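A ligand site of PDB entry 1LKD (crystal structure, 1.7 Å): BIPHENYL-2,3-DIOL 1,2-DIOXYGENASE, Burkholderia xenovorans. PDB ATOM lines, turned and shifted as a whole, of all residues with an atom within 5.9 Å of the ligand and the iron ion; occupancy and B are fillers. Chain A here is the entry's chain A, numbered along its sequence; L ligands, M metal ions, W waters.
OH of Tyr 249 sits close to O1 of the ligand, at 2.7 Å.
NE2 of His 194 lies close to O2 of the ligand.
The side-chain carboxylate of Glu 259 is in hydrogen-bond range of the side-chain hydroxyl of Tyr 249 (3.1 Å).
OE2 of Glu 259 is in hydrogen-bond range of NE2 of His 240, 2.6 Å away.
A ring nitrogen (NE2) of His 194 lies close to a ring nitrogen (ND1) of His 145, 3.3 Å away.
A ring nitrogen (ND1) of His 209 is in hydrogen-bond range of a ring nitrogen (ND1) of His 208 (2.7 Å).
NE2 of His 240 sits at hydrogen-bond distance from OH of Tyr 249 (2.9 Å).
N of His 208 is in hydrogen-bond range of O of Val 147 (3.0 Å).
The backbone NH of Thr 241 lies within hydrogen-bond range of the backbone carbonyl oxygen of Pro 279 (3.1 Å).
O of Ile 172 sits at hydrogen-bond distance from N of Ala 184 (2.8 Å).
Val 147 touches the ligand.
Ile 172 touches the ligand (CD1 to C5, 3.8 Å).
Met 174 touches the ligand.
Phe 186 touches the ligand.
Phe 201 touches the ligand (CE2 to C9, 3.7 Å).
CE1 of His 240 touches CL2 of the ligand, at 3.3 Å.
OD1 of Asn 242 touches C5 of the ligand (3.3 Å).
Pro 279 touches the ligand.
Within 4 Å of the ligand: His 145, Val 147, Ile 172, Met 174, Phe 186, His 194, Phe 201, His 209, His 240, Asn 242, Tyr 249, Glu 259 and Pro 279.
Merely in contact with the iron ion: Tyr 249 (3.8 Å).
Four residues have an atom within 4 Å of the iron ion: His 145, His 209, Tyr 249 and Glu 259.
O1 of the ligand is bound to the iron ion (2.1 Å).
The iron ion is bound by OE1 of Glu 259 (2.1 Å).
O2 of the ligand is bound to the iron ion (2.3 Å).
A ring nitrogen (NE2) of His 145 is bound to the iron ion (2.3 Å).
NE2 of His 209 binds the iron ion (2.3 Å).
The iron ion is bound by water W1 (2.4 Å).
The iron ion has six donor atoms within binding distance.
Water W2 bridges the side-chain carboxylate of Asp 243 (2.7 Å) and the side-chain carboxylate of Glu 259 (3.3 Å).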
ATOM      1  N   HIS A 145     -23.715   2.537  25.956  1.00  0.00           N
ATOM      2  CA  HIS A 145     -25.036   3.160  25.906  1.00  0.00           C
ATOM      3  C   HIS A 145     -26.151   2.166  26.183  1.00  0.00           C
ATOM      4  O   HIS A 145     -25.925   0.964  26.261  1.00  0.00           O
ATOM      5  CB  HIS A 145     -25.289   3.830  24.536  1.00  0.00           C
ATOM      6  CG  HIS A 145     -25.544   2.874  23.407  1.00  0.00           C
ATOM      7  ND1 HIS A 145     -24.661   2.689  22.364  1.00  0.00           N
ATOM      8  CD2 HIS A 145     -26.615   2.083  23.126  1.00  0.00           C
ATOM      9  CE1 HIS A 145     -25.167   1.834  21.496  1.00  0.00           C
ATOM     10  NE2 HIS A 145     -26.346   1.448  21.939  1.00  0.00           N
ATOM     11  N   VAL A 147     -30.735   1.885  25.573  1.00  0.00           N
ATOM     12  CA  VAL A 147     -31.908   2.479  24.958  1.00  0.00           C
ATOM     13  C   VAL A 147     -33.076   2.434  25.930  1.00  0.00           C
ATOM     14  O   VAL A 147     -33.572   1.366  26.274  1.00  0.00           O
ATOM     15  CB  VAL A 147     -32.266   1.714  23.677  1.00  0.00           C
ATOM     16  CG1 VAL A 147     -33.449   2.391  22.989  1.00  0.00           C
ATOM     17  CG2 VAL A 147     -31.059   1.663  22.766  1.00  0.00           C
ATOM     18  N   ILE A 172     -33.845   8.372  14.053  1.00  0.00           N
ATOM     19  CA  ILE A 172     -34.104   7.313  13.097  1.00  0.00           C
ATOM     20  C   ILE A 172     -35.576   6.964  13.232  1.00  0.00           C
ATOM     21  O   ILE A 172     -36.047   6.622  14.306  1.00  0.00           O
ATOM     22  CB  ILE A 172     -33.268   6.042  13.375  1.00  0.00           C
ATOM     23  CG1 ILE A 172     -31.777   6.357  13.228  1.00  0.00           C
ATOM     24  CG2 ILE A 172     -33.651   4.947  12.386  1.00  0.00           C
ATOM     25  CD1 ILE A 172     -30.866   5.183  13.562  1.00  0.00           C
ATOM     26  N   MET A 174     -37.959   4.485  12.936  1.00  0.00           N
ATOM     27  CA  MET A 174     -38.029   3.032  12.897  1.00  0.00           C
ATOM     28  C   MET A 174     -39.339   2.493  12.356  1.00  0.00           C
ATOM     29  O   MET A 174     -40.391   2.724  12.945  1.00  0.00           O
ATOM     30  CB  MET A 174     -37.821   2.474  14.304  1.00  0.00           C
ATOM     31  CG  MET A 174     -36.573   2.973  15.005  1.00  0.00           C
ATOM     32  SD  MET A 174     -35.090   2.134  14.463  1.00  0.00           S
ATOM     33  CE  MET A 174     -34.082   2.260  15.935  1.00  0.00           C
ATOM     34  N   ALA A 184     -36.713   7.169  16.999  1.00  0.00           N
ATOM     35  CA  ALA A 184     -35.746   6.807  18.018  1.00  0.00           C
ATOM     36  C   ALA A 184     -34.765   7.981  18.048  1.00  0.00           C
ATOM     37  O   ALA A 184     -34.257   8.389  17.006  1.00  0.00           O
ATOM     38  CB  ALA A 184     -35.025   5.510  17.645  1.00  0.00           C
ATOM     39  N   PHE A 186     -31.193   9.604  19.417  1.00  0.00           N
ATOM     40  CA  PHE A 186     -29.876   9.219  19.915  1.00  0.00           C
ATOM     41  C   PHE A 186     -29.206  10.458  20.471  1.00  0.00           C
ATOM     42  O   PHE A 186     -29.052  11.457  19.765  1.00  0.00           O
ATOM     43  CB  PHE A 186     -29.072   8.581  18.780  1.00  0.00           C
ATOM     44  CG  PHE A 186     -29.727   7.346  18.237  1.00  0.00           C
ATOM     45  CD1 PHE A 186     -30.835   7.448  17.391  1.00  0.00           C
ATOM     46  CD2 PHE A 186     -29.297   6.093  18.621  1.00  0.00           C
ATOM     47  CE1 PHE A 186     -31.498   6.310  16.954  1.00  0.00           C
ATOM     48  CE2 PHE A 186     -29.958   4.941  18.186  1.00  0.00           C
ATOM     49  CZ  PHE A 186     -31.065   5.052  17.351  1.00  0.00           C
ATOM     50  N   HIS A 194     -23.667   8.160  20.830  1.00  0.00           N
ATOM     51  CA  HIS A 194     -24.785   8.246  21.753  1.00  0.00           C
ATOM     52  C   HIS A 194     -24.504   7.422  22.995  1.00  0.00           C
ATOM     53  O   HIS A 194     -23.889   6.360  22.925  1.00  0.00           O
ATOM     54  CB  HIS A 194     -26.155   7.853  21.115  1.00  0.00           C
ATOM     55  CG  HIS A 194     -26.245   6.429  20.656  1.00  0.00           C
ATOM     56  ND1 HIS A 194     -25.672   5.990  19.482  1.00  0.00           N
ATOM     57  CD2 HIS A 194     -26.915   5.369  21.168  1.00  0.00           C
ATOM     58  CE1 HIS A 194     -25.979   4.716  19.295  1.00  0.00           C
ATOM     59  NE2 HIS A 194     -26.731   4.319  20.304  1.00  0.00           N
ATOM     60  N   ALA A 197     -30.330   6.391  24.088  1.00  0.00           N
ATOM     61  CA  ALA A 197     -31.274   6.467  22.983  1.00  0.00           C
ATOM     62  C   ALA A 197     -32.643   6.401  23.649  1.00  0.00           C
ATOM     63  O   ALA A 197     -32.789   5.810  24.713  1.00  0.00           O
ATOM     64  CB  ALA A 197     -31.080   5.306  22.015  1.00  0.00           C
ATOM     65  N   PHE A 201     -41.085   1.980  22.225  1.00  0.00           N
ATOM     66  CA  PHE A 201     -41.239   0.627  21.712  1.00  0.00           C
ATOM     67  C   PHE A 201     -42.223  -0.166  22.572  1.00  0.00           C
ATOM     68  O   PHE A 201     -42.380   0.126  23.757  1.00  0.00           O
ATOM     69  CB  PHE A 201     -39.910  -0.129  21.711  1.00  0.00           C
ATOM     70  CG  PHE A 201     -38.861   0.459  20.802  1.00  0.00           C
ATOM     71  CD1 PHE A 201     -39.198   0.957  19.545  1.00  0.00           C
ATOM     72  CD2 PHE A 201     -37.523   0.482  21.193  1.00  0.00           C
ATOM     73  CE1 PHE A 201     -38.222   1.454  18.684  1.00  0.00           C
ATOM     74  CE2 PHE A 201     -36.536   0.987  20.332  1.00  0.00           C
ATOM     75  CZ  PHE A 201     -36.888   1.470  19.080  1.00  0.00           C
ATOM     76  N   HIS A 208     -34.341  -1.490  25.976  1.00  0.00           N
ATOM     77  CA  HIS A 208     -34.383  -2.500  24.928  1.00  0.00           C
ATOM     78  C   HIS A 208     -33.065  -3.269  25.021  1.00  0.00           C
ATOM     79  O   HIS A 208     -33.044  -4.494  24.968  1.00  0.00           O
ATOM     80  CB  HIS A 208     -34.529  -1.828  23.557  1.00  0.00           C
ATOM     81  CG  HIS A 208     -34.402  -2.775  22.404  1.00  0.00           C
ATOM     82  ND1 HIS A 208     -33.185  -3.134  21.862  1.00  0.00           N
ATOM     83  CD2 HIS A 208     -35.340  -3.457  21.706  1.00  0.00           C
ATOM     84  CE1 HIS A 208     -33.377  -3.992  20.882  1.00  0.00           C
ATOM     85  NE2 HIS A 208     -34.677  -4.209  20.765  1.00  0.00           N
ATOM     86  N   HIS A 209     -31.964  -2.532  25.158  1.00  0.00           N
ATOM     87  CA  HIS A 209     -30.655  -3.155  25.283  1.00  0.00           C
ATOM     88  C   HIS A 209     -29.634  -2.175  25.832  1.00  0.00           C
ATOM     89  O   HIS A 209     -29.888  -0.975  25.897  1.00  0.00           O
ATOM     90  CB  HIS A 209     -30.132  -3.637  23.915  1.00  0.00           C
ATOM     91  CG  HIS A 209     -29.810  -2.535  22.955  1.00  0.00           C
ATOM     92  ND1 HIS A 209     -30.746  -1.958  22.134  1.00  0.00           N
ATOM     93  CD2 HIS A 209     -28.629  -1.929  22.665  1.00  0.00           C
ATOM     94  CE1 HIS A 209     -30.172  -1.042  21.370  1.00  0.00           C
ATOM     95  NE2 HIS A 209     -28.883  -1.000  21.672  1.00  0.00           N
ATOM     96  N   MET A 211     -25.291  -1.468  25.499  1.00  0.00           N
ATOM     97  CA  MET A 211     -24.248  -1.778  24.538  1.00  0.00           C
ATOM     98  C   MET A 211     -22.843  -1.652  25.118  1.00  0.00           C
ATOM     99  O   MET A 211     -22.567  -0.733  25.891  1.00  0.00           O
ATOM    100  CB  MET A 211     -24.383  -0.842  23.329  1.00  0.00           C
ATOM    101  CG  MET A 211     -23.437  -1.090  22.153  1.00  0.00           C
ATOM    102  SD  MET A 211     -21.746  -0.471  22.342  1.00  0.00           S
ATOM    103  CE  MET A 211     -21.993   1.237  22.504  1.00  0.00           C
ATOM    104  N   HIS A 240     -24.431   0.081  11.829  1.00  0.00           N
ATOM    105  CA  HIS A 240     -25.479   1.093  11.945  1.00  0.00           C
ATOM    106  C   HIS A 240     -25.281   2.282  11.027  1.00  0.00           C
ATOM    107  O   HIS A 240     -24.156   2.653  10.696  1.00  0.00           O
ATOM    108  CB  HIS A 240     -25.570   1.588  13.386  1.00  0.00           C
ATOM    109  CG  HIS A 240     -26.143   0.584  14.328  1.00  0.00           C
ATOM    110  ND1 HIS A 240     -27.415   0.074  14.185  1.00  0.00           N
ATOM    111  CD2 HIS A 240     -25.618   0.002  15.438  1.00  0.00           C
ATOM    112  CE1 HIS A 240     -27.649  -0.777  15.159  1.00  0.00           C
ATOM    113  NE2 HIS A 240     -26.576  -0.843  15.927  1.00  0.00           N
ATOM    114  N   THR A 241     -26.391   2.880  10.617  1.00  0.00           N
ATOM    115  CA  THR A 241     -26.362   4.042   9.730  1.00  0.00           C
ATOM    116  C   THR A 241     -25.887   5.304  10.427  1.00  0.00           C
ATOM    117  O   THR A 241     -25.251   6.161   9.809  1.00  0.00           O
ATOM    118  CB  THR A 241     -27.764   4.330   9.186  1.00  0.00           C
ATOM    119  OG1 THR A 241     -28.684   4.379  10.279  1.00  0.00           O
ATOM    120  CG2 THR A 241     -28.191   3.257   8.196  1.00  0.00           C
ATOM    121  N   ASN A 242     -26.197   5.443  11.722  1.00  0.00           N
ATOM    122  CA  ASN A 242     -25.837   6.667  12.422  1.00  0.00           C
ATOM    123  C   ASN A 242     -24.481   6.691  13.117  1.00  0.00           C
ATOM    124  O   ASN A 242     -23.706   7.611  12.882  1.00  0.00           O
ATOM    125  CB  ASN A 242     -26.956   7.083  13.394  1.00  0.00           C
ATOM    126  CG  ASN A 242     -27.305   6.021  14.435  1.00  0.00           C
ATOM    127  OD1 ASN A 242     -26.833   4.890  14.380  1.00  0.00           O
ATOM    128  ND2 ASN A 242     -28.143   6.403  15.388  1.00  0.00           N
ATOM    129  N   ASP A 243     -24.175   5.702  13.959  1.00  0.00           N
ATOM    130  CA  ASP A 243     -22.877   5.721  14.614  1.00  0.00           C
ATOM    131  C   ASP A 243     -21.854   4.839  13.899  1.00  0.00           C
ATOM    132  O   ASP A 243     -20.693   4.800  14.294  1.00  0.00           O
ATOM    133  CB  ASP A 243     -23.013   5.329  16.090  1.00  0.00           C
ATOM    134  CG  ASP A 243     -23.270   3.855  16.289  1.00  0.00           C
ATOM    135  OD1 ASP A 243     -23.617   3.155  15.318  1.00  0.00           O
ATOM    136  OD2 ASP A 243     -23.118   3.398  17.453  1.00  0.00           O
ATOM    137  N   TYR A 249     -26.639  -8.340  18.121  1.00  0.00           N
ATOM    138  CA  TYR A 249     -27.442  -8.261  19.335  1.00  0.00           C
ATOM    139  C   TYR A 249     -27.713  -9.673  19.841  1.00  0.00           C
ATOM    140  O   TYR A 249     -27.764 -10.625  19.066  1.00  0.00           O
ATOM    141  CB  TYR A 249     -28.782  -7.572  19.072  1.00  0.00           C
ATOM    142  CG  TYR A 249     -28.666  -6.118  18.685  1.00  0.00           C
ATOM    143  CD1 TYR A 249     -28.285  -5.735  17.393  1.00  0.00           C
ATOM    144  CD2 TYR A 249     -28.996  -5.114  19.590  1.00  0.00           C
ATOM    145  CE1 TYR A 249     -28.240  -4.397  17.027  1.00  0.00           C
ATOM    146  CE2 TYR A 249     -28.949  -3.767  19.235  1.00  0.00           C
ATOM    147  CZ  TYR A 249     -28.567  -3.419  17.952  1.00  0.00           C
ATOM    148  OH  TYR A 249     -28.561  -2.100  17.590  1.00  0.00           O
ATOM    149  N   GLU A 259     -26.016  -5.302  23.051  1.00  0.00           N
ATOM    150  CA  GLU A 259     -25.418  -5.054  21.749  1.00  0.00           C
ATOM    151  C   GLU A 259     -23.914  -5.087  22.011  1.00  0.00           C
ATOM    152  O   GLU A 259     -23.436  -4.518  22.991  1.00  0.00           O
ATOM    153  CB  GLU A 259     -25.840  -3.703  21.204  1.00  0.00           C
ATOM    154  CG  GLU A 259     -25.183  -3.369  19.887  1.00  0.00           C
ATOM    155  CD  GLU A 259     -25.664  -2.068  19.300  1.00  0.00           C
ATOM    156  OE1 GLU A 259     -26.222  -1.237  20.052  1.00  0.00           O
ATOM    157  OE2 GLU A 259     -25.473  -1.856  18.075  1.00  0.00           O
ATOM    158  N   PRO A 279     -32.024   1.857  10.447  1.00  0.00           N
ATOM    159  CA  PRO A 279     -31.021   1.857  11.510  1.00  0.00           C
ATOM    160  C   PRO A 279     -29.734   1.122  11.118  1.00  0.00           C
ATOM    161  O   PRO A 279     -28.730   1.211  11.828  1.00  0.00           O
ATOM    162  CB  PRO A 279     -31.739   1.164  12.657  1.00  0.00           C
ATOM    163  CG  PRO A 279     -32.495   0.095  11.935  1.00  0.00           C
ATOM    164  CD  PRO A 279     -33.059   0.831  10.718  1.00  0.00           C
ATOM    165  N   SER A 280     -29.767   0.408  10.006  1.00  0.00           N
ATOM    166  CA  SER A 280     -28.596  -0.363   9.570  1.00  0.00           C
ATOM    167  C   SER A 280     -28.218  -0.195   8.094  1.00  0.00           C
ATOM    168  O   SER A 280     -29.082  -0.262   7.216  1.00  0.00           O
ATOM    169  CB  SER A 280     -28.831  -1.846   9.854  1.00  0.00           C
ATOM    170  OG  SER A 280     -29.147  -2.053  11.223  1.00  0.00           O
ATOM    171  N   HIS A 284     -27.563  -6.895  10.432  1.00  0.00           N
ATOM    172  CA  HIS A 284     -28.518  -6.724  11.515  1.00  0.00           C
ATOM    173  C   HIS A 284     -29.861  -7.342  11.142  1.00  0.00           C
ATOM    174  O   HIS A 284     -30.930  -6.772  11.392  1.00  0.00           O
ATOM    175  CB  HIS A 284     -28.691  -5.250  11.860  1.00  0.00           C
ATOM    176  CG  HIS A 284     -27.540  -4.679  12.637  1.00  0.00           C
ATOM    177  ND1 HIS A 284     -27.200  -3.346  12.601  1.00  0.00           N
ATOM    178  CD2 HIS A 284     -26.667  -5.268  13.488  1.00  0.00           C
ATOM    179  CE1 HIS A 284     -26.169  -3.135  13.401  1.00  0.00           C
ATOM    180  NE2 HIS A 284     -25.824  -4.288  13.948  1.00  0.00           N
HETATM  181  C1  LIG L   1     -30.184   1.095  17.028  1.00  0.00           C
HETATM  182  C2  LIG L   1     -29.062   0.987  17.876  1.00  0.00           C
HETATM  183  O1  LIG L   1     -29.060   0.155  18.961  1.00  0.00           O
HETATM  184  C3  LIG L   1     -27.885   1.730  17.659  1.00  0.00           C
HETATM  185  O2  LIG L   1     -26.845   1.566  18.556  1.00  0.00           O
HETATM  186  C4  LIG L   1     -27.815   2.622  16.552  1.00  0.00           C
HETATM  187  C5  LIG L   1     -28.931   2.735  15.682  1.00  0.00           C
HETATM  188  C6  LIG L   1     -30.112   1.972  15.923  1.00  0.00           C
HETATM  189  C7  LIG L   1     -31.415   0.268  17.329  1.00  0.00           C
HETATM  190  C8  LIG L   1     -32.252   0.609  18.432  1.00  0.00           C
HETATM  191  C9  LIG L   1     -33.407  -0.155  18.752  1.00  0.00           C
HETATM  192  C10 LIG L   1     -33.759  -1.273  17.967  1.00  0.00           C
HETATM  193  C11 LIG L   1     -32.949  -1.625  16.868  1.00  0.00           C
HETATM  194  C12 LIG L   1     -31.794  -0.861  16.548  1.00  0.00           C
HETATM  195 CL1  LIG L   1     -31.976   1.971  19.500  1.00  0.00          CL
HETATM  196 CL2  LIG L   1     -30.925  -1.447  15.152  1.00  0.00          CL
HETATM  197 FE    FE M   1     -27.541   0.324  20.342  1.00  0.00          FE
HETATM  198  O   HOH W   1     -28.847   2.317  20.760  1.00  0.00           O
HETATM  199  O   HOH W   2     -23.971   1.099  18.492  1.00  0.00           O
